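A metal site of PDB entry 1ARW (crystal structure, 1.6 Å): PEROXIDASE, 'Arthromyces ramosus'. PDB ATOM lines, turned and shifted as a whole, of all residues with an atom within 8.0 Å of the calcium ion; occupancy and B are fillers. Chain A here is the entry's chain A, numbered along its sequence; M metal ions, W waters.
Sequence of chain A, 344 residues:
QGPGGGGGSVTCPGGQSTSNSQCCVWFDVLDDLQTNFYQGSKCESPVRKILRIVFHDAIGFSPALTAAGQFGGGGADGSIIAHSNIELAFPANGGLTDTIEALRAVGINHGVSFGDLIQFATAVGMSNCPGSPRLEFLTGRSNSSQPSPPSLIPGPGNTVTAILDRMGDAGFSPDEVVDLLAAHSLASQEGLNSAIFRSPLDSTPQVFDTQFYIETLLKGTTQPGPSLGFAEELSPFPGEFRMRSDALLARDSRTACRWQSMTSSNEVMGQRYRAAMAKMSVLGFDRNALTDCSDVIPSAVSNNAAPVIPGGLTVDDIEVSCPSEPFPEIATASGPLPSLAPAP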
ATOM      1  N   ILE A  53       9.123  -9.608  27.542  1.00  0.00           N
ATOM      2  CA  ILE A  53       7.800  -9.795  26.980  1.00  0.00           C
ATOM      3  C   ILE A  53       7.653 -11.077  26.161  1.00  0.00           C
ATOM      4  O   ILE A  53       6.650 -11.765  26.319  1.00  0.00           O
ATOM      5  CB  ILE A  53       7.473  -8.537  26.136  1.00  0.00           C
ATOM      6  CG1 ILE A  53       7.227  -7.338  27.075  1.00  0.00           C
ATOM      7  CG2 ILE A  53       6.217  -8.784  25.284  1.00  0.00           C
ATOM      8  CD1 ILE A  53       7.138  -6.035  26.244  1.00  0.00           C
ATOM      9  N   VAL A  54       8.580 -11.456  25.270  1.00  0.00           N
ATOM     10  CA  VAL A  54       8.406 -12.661  24.477  1.00  0.00           C
ATOM     11  C   VAL A  54       8.383 -13.885  25.386  1.00  0.00           C
ATOM     12  O   VAL A  54       7.575 -14.782  25.166  1.00  0.00           O
ATOM     13  CB  VAL A  54       9.546 -12.676  23.423  1.00  0.00           C
ATOM     14  CG1 VAL A  54      10.921 -13.032  24.006  1.00  0.00           C
ATOM     15  CG2 VAL A  54       9.126 -13.650  22.349  1.00  0.00           C
ATOM     16  N   PHE A  55       9.188 -13.895  26.469  1.00  0.00           N
ATOM     17  CA  PHE A  55       9.238 -14.981  27.421  1.00  0.00           C
ATOM     18  C   PHE A  55       7.916 -14.962  28.175  1.00  0.00           C
ATOM     19  O   PHE A  55       7.233 -15.979  28.189  1.00  0.00           O
ATOM     20  CB  PHE A  55      10.434 -14.779  28.410  1.00  0.00           C
ATOM     21  CG  PHE A  55      10.539 -15.774  29.584  1.00  0.00           C
ATOM     22  CD1 PHE A  55      10.219 -17.107  29.447  1.00  0.00           C
ATOM     23  CD2 PHE A  55      10.970 -15.318  30.825  1.00  0.00           C
ATOM     24  CE1 PHE A  55      10.320 -17.970  30.511  1.00  0.00           C
ATOM     25  CE2 PHE A  55      11.071 -16.181  31.889  1.00  0.00           C
ATOM     26  CZ  PHE A  55      10.748 -17.503  31.739  1.00  0.00           C
ATOM     27  N   HIS A  56       7.480 -13.834  28.738  1.00  0.00           N
ATOM     28  CA  HIS A  56       6.238 -13.784  29.503  1.00  0.00           C
ATOM     29  C   HIS A  56       4.984 -14.075  28.696  1.00  0.00           C
ATOM     30  O   HIS A  56       3.990 -14.571  29.252  1.00  0.00           O
ATOM     31  CB  HIS A  56       6.123 -12.433  30.158  1.00  0.00           C
ATOM     32  CG  HIS A  56       7.178 -12.255  31.242  1.00  0.00           C
ATOM     33  ND1 HIS A  56       7.150 -11.310  32.170  1.00  0.00           N
ATOM     34  CD2 HIS A  56       8.331 -12.984  31.440  1.00  0.00           C
ATOM     35  CE1 HIS A  56       8.217 -11.430  32.907  1.00  0.00           C
ATOM     36  NE2 HIS A  56       8.928 -12.432  32.467  1.00  0.00           N
ATOM     37  N   ASP A  57       5.026 -13.797  27.394  1.00  0.00           N
ATOM     38  CA  ASP A  57       3.915 -14.138  26.522  1.00  0.00           C
ATOM     39  C   ASP A  57       3.886 -15.650  26.238  1.00  0.00           C
ATOM     40  O   ASP A  57       2.845 -16.298  26.485  1.00  0.00           O
ATOM     41  CB  ASP A  57       4.008 -13.409  25.137  1.00  0.00           C
ATOM     42  CG  ASP A  57       2.831 -13.689  24.238  1.00  0.00           C
ATOM     43  OD1 ASP A  57       1.724 -13.952  24.742  1.00  0.00           O
ATOM     44  OD2 ASP A  57       3.004 -13.688  23.033  1.00  0.00           O
ATOM     45  N   ALA A  58       5.016 -16.208  25.813  1.00  0.00           N
ATOM     46  CA  ALA A  58       5.068 -17.594  25.404  1.00  0.00           C
ATOM     47  C   ALA A  58       4.964 -18.590  26.528  1.00  0.00           C
ATOM     48  O   ALA A  58       4.339 -19.649  26.369  1.00  0.00           O
ATOM     49  CB  ALA A  58       6.371 -17.854  24.645  1.00  0.00           C
ATOM     50  N   ILE A  59       5.485 -18.288  27.718  1.00  0.00           N
ATOM     51  CA  ILE A  59       5.417 -19.230  28.812  1.00  0.00           C
ATOM     52  C   ILE A  59       4.020 -19.360  29.422  1.00  0.00           C
ATOM     53  O   ILE A  59       3.849 -20.223  30.282  1.00  0.00           O
ATOM     54  CB  ILE A  59       6.545 -18.813  29.840  1.00  0.00           C
ATOM     55  CG1 ILE A  59       7.032 -20.075  30.576  1.00  0.00           C
ATOM     56  CG2 ILE A  59       6.049 -17.757  30.832  1.00  0.00           C
ATOM     57  CD1 ILE A  59       7.733 -21.091  29.660  1.00  0.00           C
ATOM     58  N   GLY A  60       2.997 -18.550  29.043  1.00  0.00           N
ATOM     59  CA  GLY A  60       1.673 -18.764  29.597  1.00  0.00           C
ATOM     60  C   GLY A  60       1.092 -19.910  28.794  1.00  0.00           C
ATOM     61  O   GLY A  60       0.216 -19.732  27.928  1.00  0.00           O
ATOM     62  N   PHE A  61       1.607 -21.105  29.041  1.00  0.00           N
ATOM     63  CA  PHE A  61       1.214 -22.293  28.317  1.00  0.00           C
ATOM     64  C   PHE A  61       1.421 -23.455  29.285  1.00  0.00           C
ATOM     65  O   PHE A  61       2.557 -23.685  29.726  1.00  0.00           O
ATOM     66  CB  PHE A  61       2.103 -22.436  27.058  1.00  0.00           C
ATOM     67  CG  PHE A  61       1.808 -23.704  26.259  1.00  0.00           C
ATOM     68  CD1 PHE A  61       0.681 -23.795  25.492  1.00  0.00           C
ATOM     69  CD2 PHE A  61       2.693 -24.759  26.317  1.00  0.00           C
ATOM     70  CE1 PHE A  61       0.426 -24.950  24.783  1.00  0.00           C
ATOM     71  CE2 PHE A  61       2.435 -25.913  25.593  1.00  0.00           C
ATOM     72  CZ  PHE A  61       1.295 -26.014  24.827  1.00  0.00           C
ATOM     73  N   GLY A  73      -3.670 -21.705  28.731  1.00  0.00           N
ATOM     74  CA  GLY A  73      -2.925 -20.616  28.093  1.00  0.00           C
ATOM     75  C   GLY A  73      -2.655 -20.918  26.626  1.00  0.00           C
ATOM     76  O   GLY A  73      -2.541 -22.096  26.260  1.00  0.00           O
ATOM     77  N   GLY A  74      -2.590 -19.929  25.767  1.00  0.00           N
ATOM     78  CA  GLY A  74      -2.381 -20.157  24.340  1.00  0.00           C
ATOM     79  C   GLY A  74      -0.913 -20.039  23.889  1.00  0.00           C
ATOM     80  O   GLY A  74      -0.672 -19.995  22.675  1.00  0.00           O
ATOM     81  N   GLY A  75       0.045 -19.909  24.813  1.00  0.00           N
ATOM     82  CA  GLY A  75       1.451 -19.821  24.449  1.00  0.00           C
ATOM     83  C   GLY A  75       1.803 -18.483  23.810  1.00  0.00           C
ATOM     84  O   GLY A  75       1.397 -17.429  24.324  1.00  0.00           O
ATOM     85  N   ALA A  76       2.516 -18.534  22.684  1.00  0.00           N
ATOM     86  CA  ALA A  76       3.009 -17.346  21.991  1.00  0.00           C
ATOM     87  C   ALA A  76       1.939 -16.692  21.130  1.00  0.00           C
ATOM     88  O   ALA A  76       2.131 -16.431  19.945  1.00  0.00           O
ATOM     89  CB  ALA A  76       4.219 -17.781  21.146  1.00  0.00           C
ATOM     90  N   ASP A  77       0.848 -16.286  21.786  1.00  0.00           N
ATOM     91  CA  ASP A  77      -0.346 -15.755  21.130  1.00  0.00           C
ATOM     92  C   ASP A  77      -0.586 -14.240  21.188  1.00  0.00           C
ATOM     93  O   ASP A  77      -1.619 -13.737  20.753  1.00  0.00           O
ATOM     94  CB  ASP A  77      -1.556 -16.533  21.734  1.00  0.00           C
ATOM     95  CG  ASP A  77      -1.730 -16.385  23.264  1.00  0.00           C
ATOM     96  OD1 ASP A  77      -0.932 -15.699  23.906  1.00  0.00           O
ATOM     97  OD2 ASP A  77      -2.669 -16.970  23.824  1.00  0.00           O
ATOM     98  N   GLY A  78       0.330 -13.487  21.787  1.00  0.00           N
ATOM     99  CA  GLY A  78       0.147 -12.041  21.951  1.00  0.00           C
ATOM    100  C   GLY A  78      -0.886 -11.691  23.009  1.00  0.00           C
ATOM    101  O   GLY A  78      -1.325 -10.534  23.070  1.00  0.00           O
ATOM    102  N   SER A  79      -1.247 -12.624  23.911  1.00  0.00           N
ATOM    103  CA  SER A  79      -2.257 -12.359  24.914  1.00  0.00           C
ATOM    104  C   SER A  79      -1.734 -11.289  25.864  1.00  0.00           C
ATOM    105  O   SER A  79      -2.567 -10.584  26.429  1.00  0.00           O
ATOM    106  CB  SER A  79      -2.591 -13.603  25.725  1.00  0.00           C
ATOM    107  OG  SER A  79      -1.435 -14.108  26.419  1.00  0.00           O
ATOM    108  N   ILE A  80      -0.411 -11.139  26.076  1.00  0.00           N
ATOM    109  CA  ILE A  80       0.076 -10.095  26.972  1.00  0.00           C
ATOM    110  C   ILE A  80      -0.252  -8.698  26.451  1.00  0.00           C
ATOM    111  O   ILE A  80      -0.334  -7.741  27.230  1.00  0.00           O
ATOM    112  CB  ILE A  80       1.628 -10.342  27.201  1.00  0.00           C
ATOM    113  CG1 ILE A  80       2.123  -9.468  28.390  1.00  0.00           C
ATOM    114  CG2 ILE A  80       2.428 -10.074  25.916  1.00  0.00           C
ATOM    115  CD1 ILE A  80       3.512  -9.810  28.935  1.00  0.00           C
ATOM    116  N   ILE A  81      -0.520  -8.520  25.152  1.00  0.00           N
ATOM    117  CA  ILE A  81      -0.917  -7.214  24.620  1.00  0.00           C
ATOM    118  C   ILE A  81      -2.443  -7.195  24.568  1.00  0.00           C
ATOM    119  O   ILE A  81      -3.068  -6.317  25.176  1.00  0.00           O
ATOM    120  CB  ILE A  81      -0.310  -6.999  23.206  1.00  0.00           C
ATOM    121  CG1 ILE A  81       1.230  -7.009  23.257  1.00  0.00           C
ATOM    122  CG2 ILE A  81      -0.826  -5.665  22.655  1.00  0.00           C
ATOM    123  CD1 ILE A  81       1.922  -6.818  21.912  1.00  0.00           C
ATOM    124  N   HIS A  83      -4.743  -8.836  26.072  1.00  0.00           N
ATOM    125  CA  HIS A  83      -5.322  -8.901  27.401  1.00  0.00           C
ATOM    126  C   HIS A  83      -4.339  -8.304  28.385  1.00  0.00           C
ATOM    127  O   HIS A  83      -4.175  -8.837  29.483  1.00  0.00           O
ATOM    128  CB  HIS A  83      -5.601 -10.326  27.811  1.00  0.00           C
ATOM    129  CG  HIS A  83      -6.556 -10.889  26.790  1.00  0.00           C
ATOM    130  ND1 HIS A  83      -7.855 -10.440  26.628  1.00  0.00           N
ATOM    131  CD2 HIS A  83      -6.230 -11.896  25.868  1.00  0.00           C
ATOM    132  CE1 HIS A  83      -8.333 -11.191  25.613  1.00  0.00           C
ATOM    133  NE2 HIS A  83      -7.436 -12.016  25.177  1.00  0.00           N
ATOM    134  N   GLU A  87      -3.132  -9.395  32.254  1.00  0.00           N
ATOM    135  CA  GLU A  87      -1.787  -9.936  32.449  1.00  0.00           C
ATOM    136  C   GLU A  87      -0.797  -8.992  33.074  1.00  0.00           C
ATOM    137  O   GLU A  87       0.102  -9.436  33.790  1.00  0.00           O
ATOM    138  CB  GLU A  87      -1.217 -10.444  31.120  1.00  0.00           C
ATOM    139  CG  GLU A  87      -1.958 -11.715  30.731  1.00  0.00           C
ATOM    140  CD  GLU A  87      -1.322 -12.447  29.557  1.00  0.00           C
ATOM    141  OE1 GLU A  87      -0.092 -12.493  29.472  1.00  0.00           O
ATOM    142  OE2 GLU A  87      -2.075 -12.985  28.754  1.00  0.00           O
ATOM    143  N   GLY A 115       0.822 -11.822  18.434  1.00  0.00           N
ATOM    144  CA  GLY A 115       1.762 -12.936  18.707  1.00  0.00           C
ATOM    145  C   GLY A 115       2.919 -12.926  17.717  1.00  0.00           C
ATOM    146  O   GLY A 115       4.082 -13.068  18.089  1.00  0.00           O
ATOM    147  N   ILE A 118       5.332  -9.764  18.400  1.00  0.00           N
ATOM    148  CA  ILE A 118       6.291  -9.922  19.500  1.00  0.00           C
ATOM    149  C   ILE A 118       7.498 -10.739  19.074  1.00  0.00           C
ATOM    150  O   ILE A 118       8.640 -10.373  19.382  1.00  0.00           O
ATOM    151  CB  ILE A 118       5.561 -10.554  20.718  1.00  0.00           C
ATOM    152  CG1 ILE A 118       4.560  -9.545  21.311  1.00  0.00           C
ATOM    153  CG2 ILE A 118       6.590 -10.918  21.793  1.00  0.00           C
ATOM    154  CD1 ILE A 118       3.731 -10.134  22.464  1.00  0.00           C
ATOM    155  N   SER A 145      -6.820 -14.482  21.130  1.00  0.00           N
ATOM    156  CA  SER A 145      -6.236 -15.130  22.301  1.00  0.00           C
ATOM    157  C   SER A 145      -7.131 -14.983  23.518  1.00  0.00           C
ATOM    158  O   SER A 145      -8.059 -14.167  23.526  1.00  0.00           O
ATOM    159  CB  SER A 145      -4.876 -14.519  22.643  1.00  0.00           C
ATOM    160  OG  SER A 145      -5.030 -13.122  22.797  1.00  0.00           O
ATOM    161  N   GLN A 146      -6.944 -15.846  24.495  1.00  0.00           N
ATOM    162  CA  GLN A 146      -7.648 -15.758  25.767  1.00  0.00           C
ATOM    163  C   GLN A 146      -6.562 -15.277  26.736  1.00  0.00           C
ATOM    164  O   GLN A 146      -5.378 -15.453  26.431  1.00  0.00           O
ATOM    165  CB  GLN A 146      -8.132 -17.119  26.175  1.00  0.00           C
ATOM    166  CG  GLN A 146      -9.412 -17.430  25.458  1.00  0.00           C
ATOM    167  CD  GLN A 146      -9.704 -18.925  25.445  1.00  0.00           C
ATOM    168  OE1 GLN A 146     -10.267 -19.515  26.392  1.00  0.00           O
ATOM    169  NE2 GLN A 146      -9.303 -19.527  24.317  1.00  0.00           N
ATOM    170  N   PRO A 147      -6.870 -14.665  27.906  1.00  0.00           N
ATOM    171  CA  PRO A 147      -5.877 -14.226  28.867  1.00  0.00           C
ATOM    172  C   PRO A 147      -5.113 -15.419  29.387  1.00  0.00           C
ATOM    173  O   PRO A 147      -5.680 -16.488  29.563  1.00  0.00           O
ATOM    174  CB  PRO A 147      -6.637 -13.541  29.972  1.00  0.00           C
ATOM    175  CG  PRO A 147      -7.978 -13.250  29.356  1.00  0.00           C
ATOM    176  CD  PRO A 147      -8.205 -14.424  28.431  1.00  0.00           C
ATOM    177  N   SER A 148      -3.816 -15.262  29.619  1.00  0.00           N
ATOM    178  CA  SER A 148      -3.034 -16.310  30.206  1.00  0.00           C
ATOM    179  C   SER A 148      -3.554 -16.592  31.614  1.00  0.00           C
ATOM    180  O   SER A 148      -4.043 -15.689  32.309  1.00  0.00           O
ATOM    181  CB  SER A 148      -1.557 -15.903  30.299  1.00  0.00           C
ATOM    182  OG  SER A 148      -0.740 -16.824  31.037  1.00  0.00           O
ATOM    183  N   PRO A 149      -3.521 -17.834  32.093  1.00  0.00           N
ATOM    184  CA  PRO A 149      -3.797 -18.157  33.482  1.00  0.00           C
ATOM    185  C   PRO A 149      -2.705 -17.493  34.330  1.00  0.00           C
ATOM    186  O   PRO A 149      -1.586 -17.261  33.843  1.00  0.00           O
ATOM    187  CB  PRO A 149      -3.770 -19.654  33.485  1.00  0.00           C
ATOM    188  CG  PRO A 149      -4.318 -19.983  32.139  1.00  0.00           C
ATOM    189  CD  PRO A 149      -3.481 -19.042  31.291  1.00  0.00           C
ATOM    190  N   LEU A 283       5.215 -22.270  21.000  1.00  0.00           N
ATOM    191  CA  LEU A 283       4.386 -22.877  22.029  1.00  0.00           C
ATOM    192  C   LEU A 283       2.920 -22.457  21.807  1.00  0.00           C
ATOM    193  O   LEU A 283       2.601 -21.275  21.647  1.00  0.00           O
ATOM    194  CB  LEU A 283       4.938 -22.386  23.360  1.00  0.00           C
ATOM    195  CG  LEU A 283       5.711 -23.273  24.353  1.00  0.00           C
ATOM    196  CD1 LEU A 283       6.620 -24.320  23.715  1.00  0.00           C
ATOM    197  CD2 LEU A 283       6.410 -22.284  25.257  1.00  0.00           C
ATOM    198  N   PHE A 285       1.248 -23.547  19.149  1.00  0.00           N
ATOM    199  CA  PHE A 285       1.077 -23.563  17.699  1.00  0.00           C
ATOM    200  C   PHE A 285       1.762 -24.747  17.059  1.00  0.00           C
ATOM    201  O   PHE A 285       2.587 -25.454  17.656  1.00  0.00           O
ATOM    202  CB  PHE A 285       1.668 -22.303  17.010  1.00  0.00           C
ATOM    203  CG  PHE A 285       0.896 -21.072  17.447  1.00  0.00           C
ATOM    204  CD1 PHE A 285      -0.274 -20.722  16.799  1.00  0.00           C
ATOM    205  CD2 PHE A 285       1.312 -20.385  18.582  1.00  0.00           C
ATOM    206  CE1 PHE A 285      -1.042 -19.687  17.289  1.00  0.00           C
ATOM    207  CE2 PHE A 285       0.529 -19.340  19.076  1.00  0.00           C
ATOM    208  CZ  PHE A 285      -0.640 -19.001  18.427  1.00  0.00           C
HETATM  209 CA    CA M   1       0.527 -15.593  25.857  1.00  0.00          CA
HETATM  210  O   HOH W   1      -0.557 -17.272  27.193  1.00  0.00           O
HETATM  211  O   HOH W   2       1.031 -14.640  28.118  1.00  0.00           O
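The side-chain carboxylate (OD2) of Asp 57 is in hydrogen-bond range of the backbone NH (N) of Gly 78 (3.0 Å).
O of Gly 60 lies within hydrogen-bond range of N of Gly 75 (3.1 Å).
OG of Ser 79 sits close to OE2 of Glu 87, 2.7 Å away.
Water W2 bridges the side-chain carboxylate of Glu 87 and the backbone carbonyl oxygen of His 56.
The calcium ion is bound by the side-chain carboxylate (OD1) of Asp 57 (2.3 Å).
Water W1 binds the calcium ion, 2.4 Å away.
The side-chain carboxylate (OD1) of Asp 77 is bound to the calcium ion (2.4 Å).
The backbone carbonyl oxygen (O) of Asp 57 is bound to the calcium ion, at 2.5 Å.
The calcium ion is bound by water W2 (2.5 Å).
OG of Ser 79 binds the calcium ion (2.5 Å).
O of Gly 75 binds the calcium ion.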
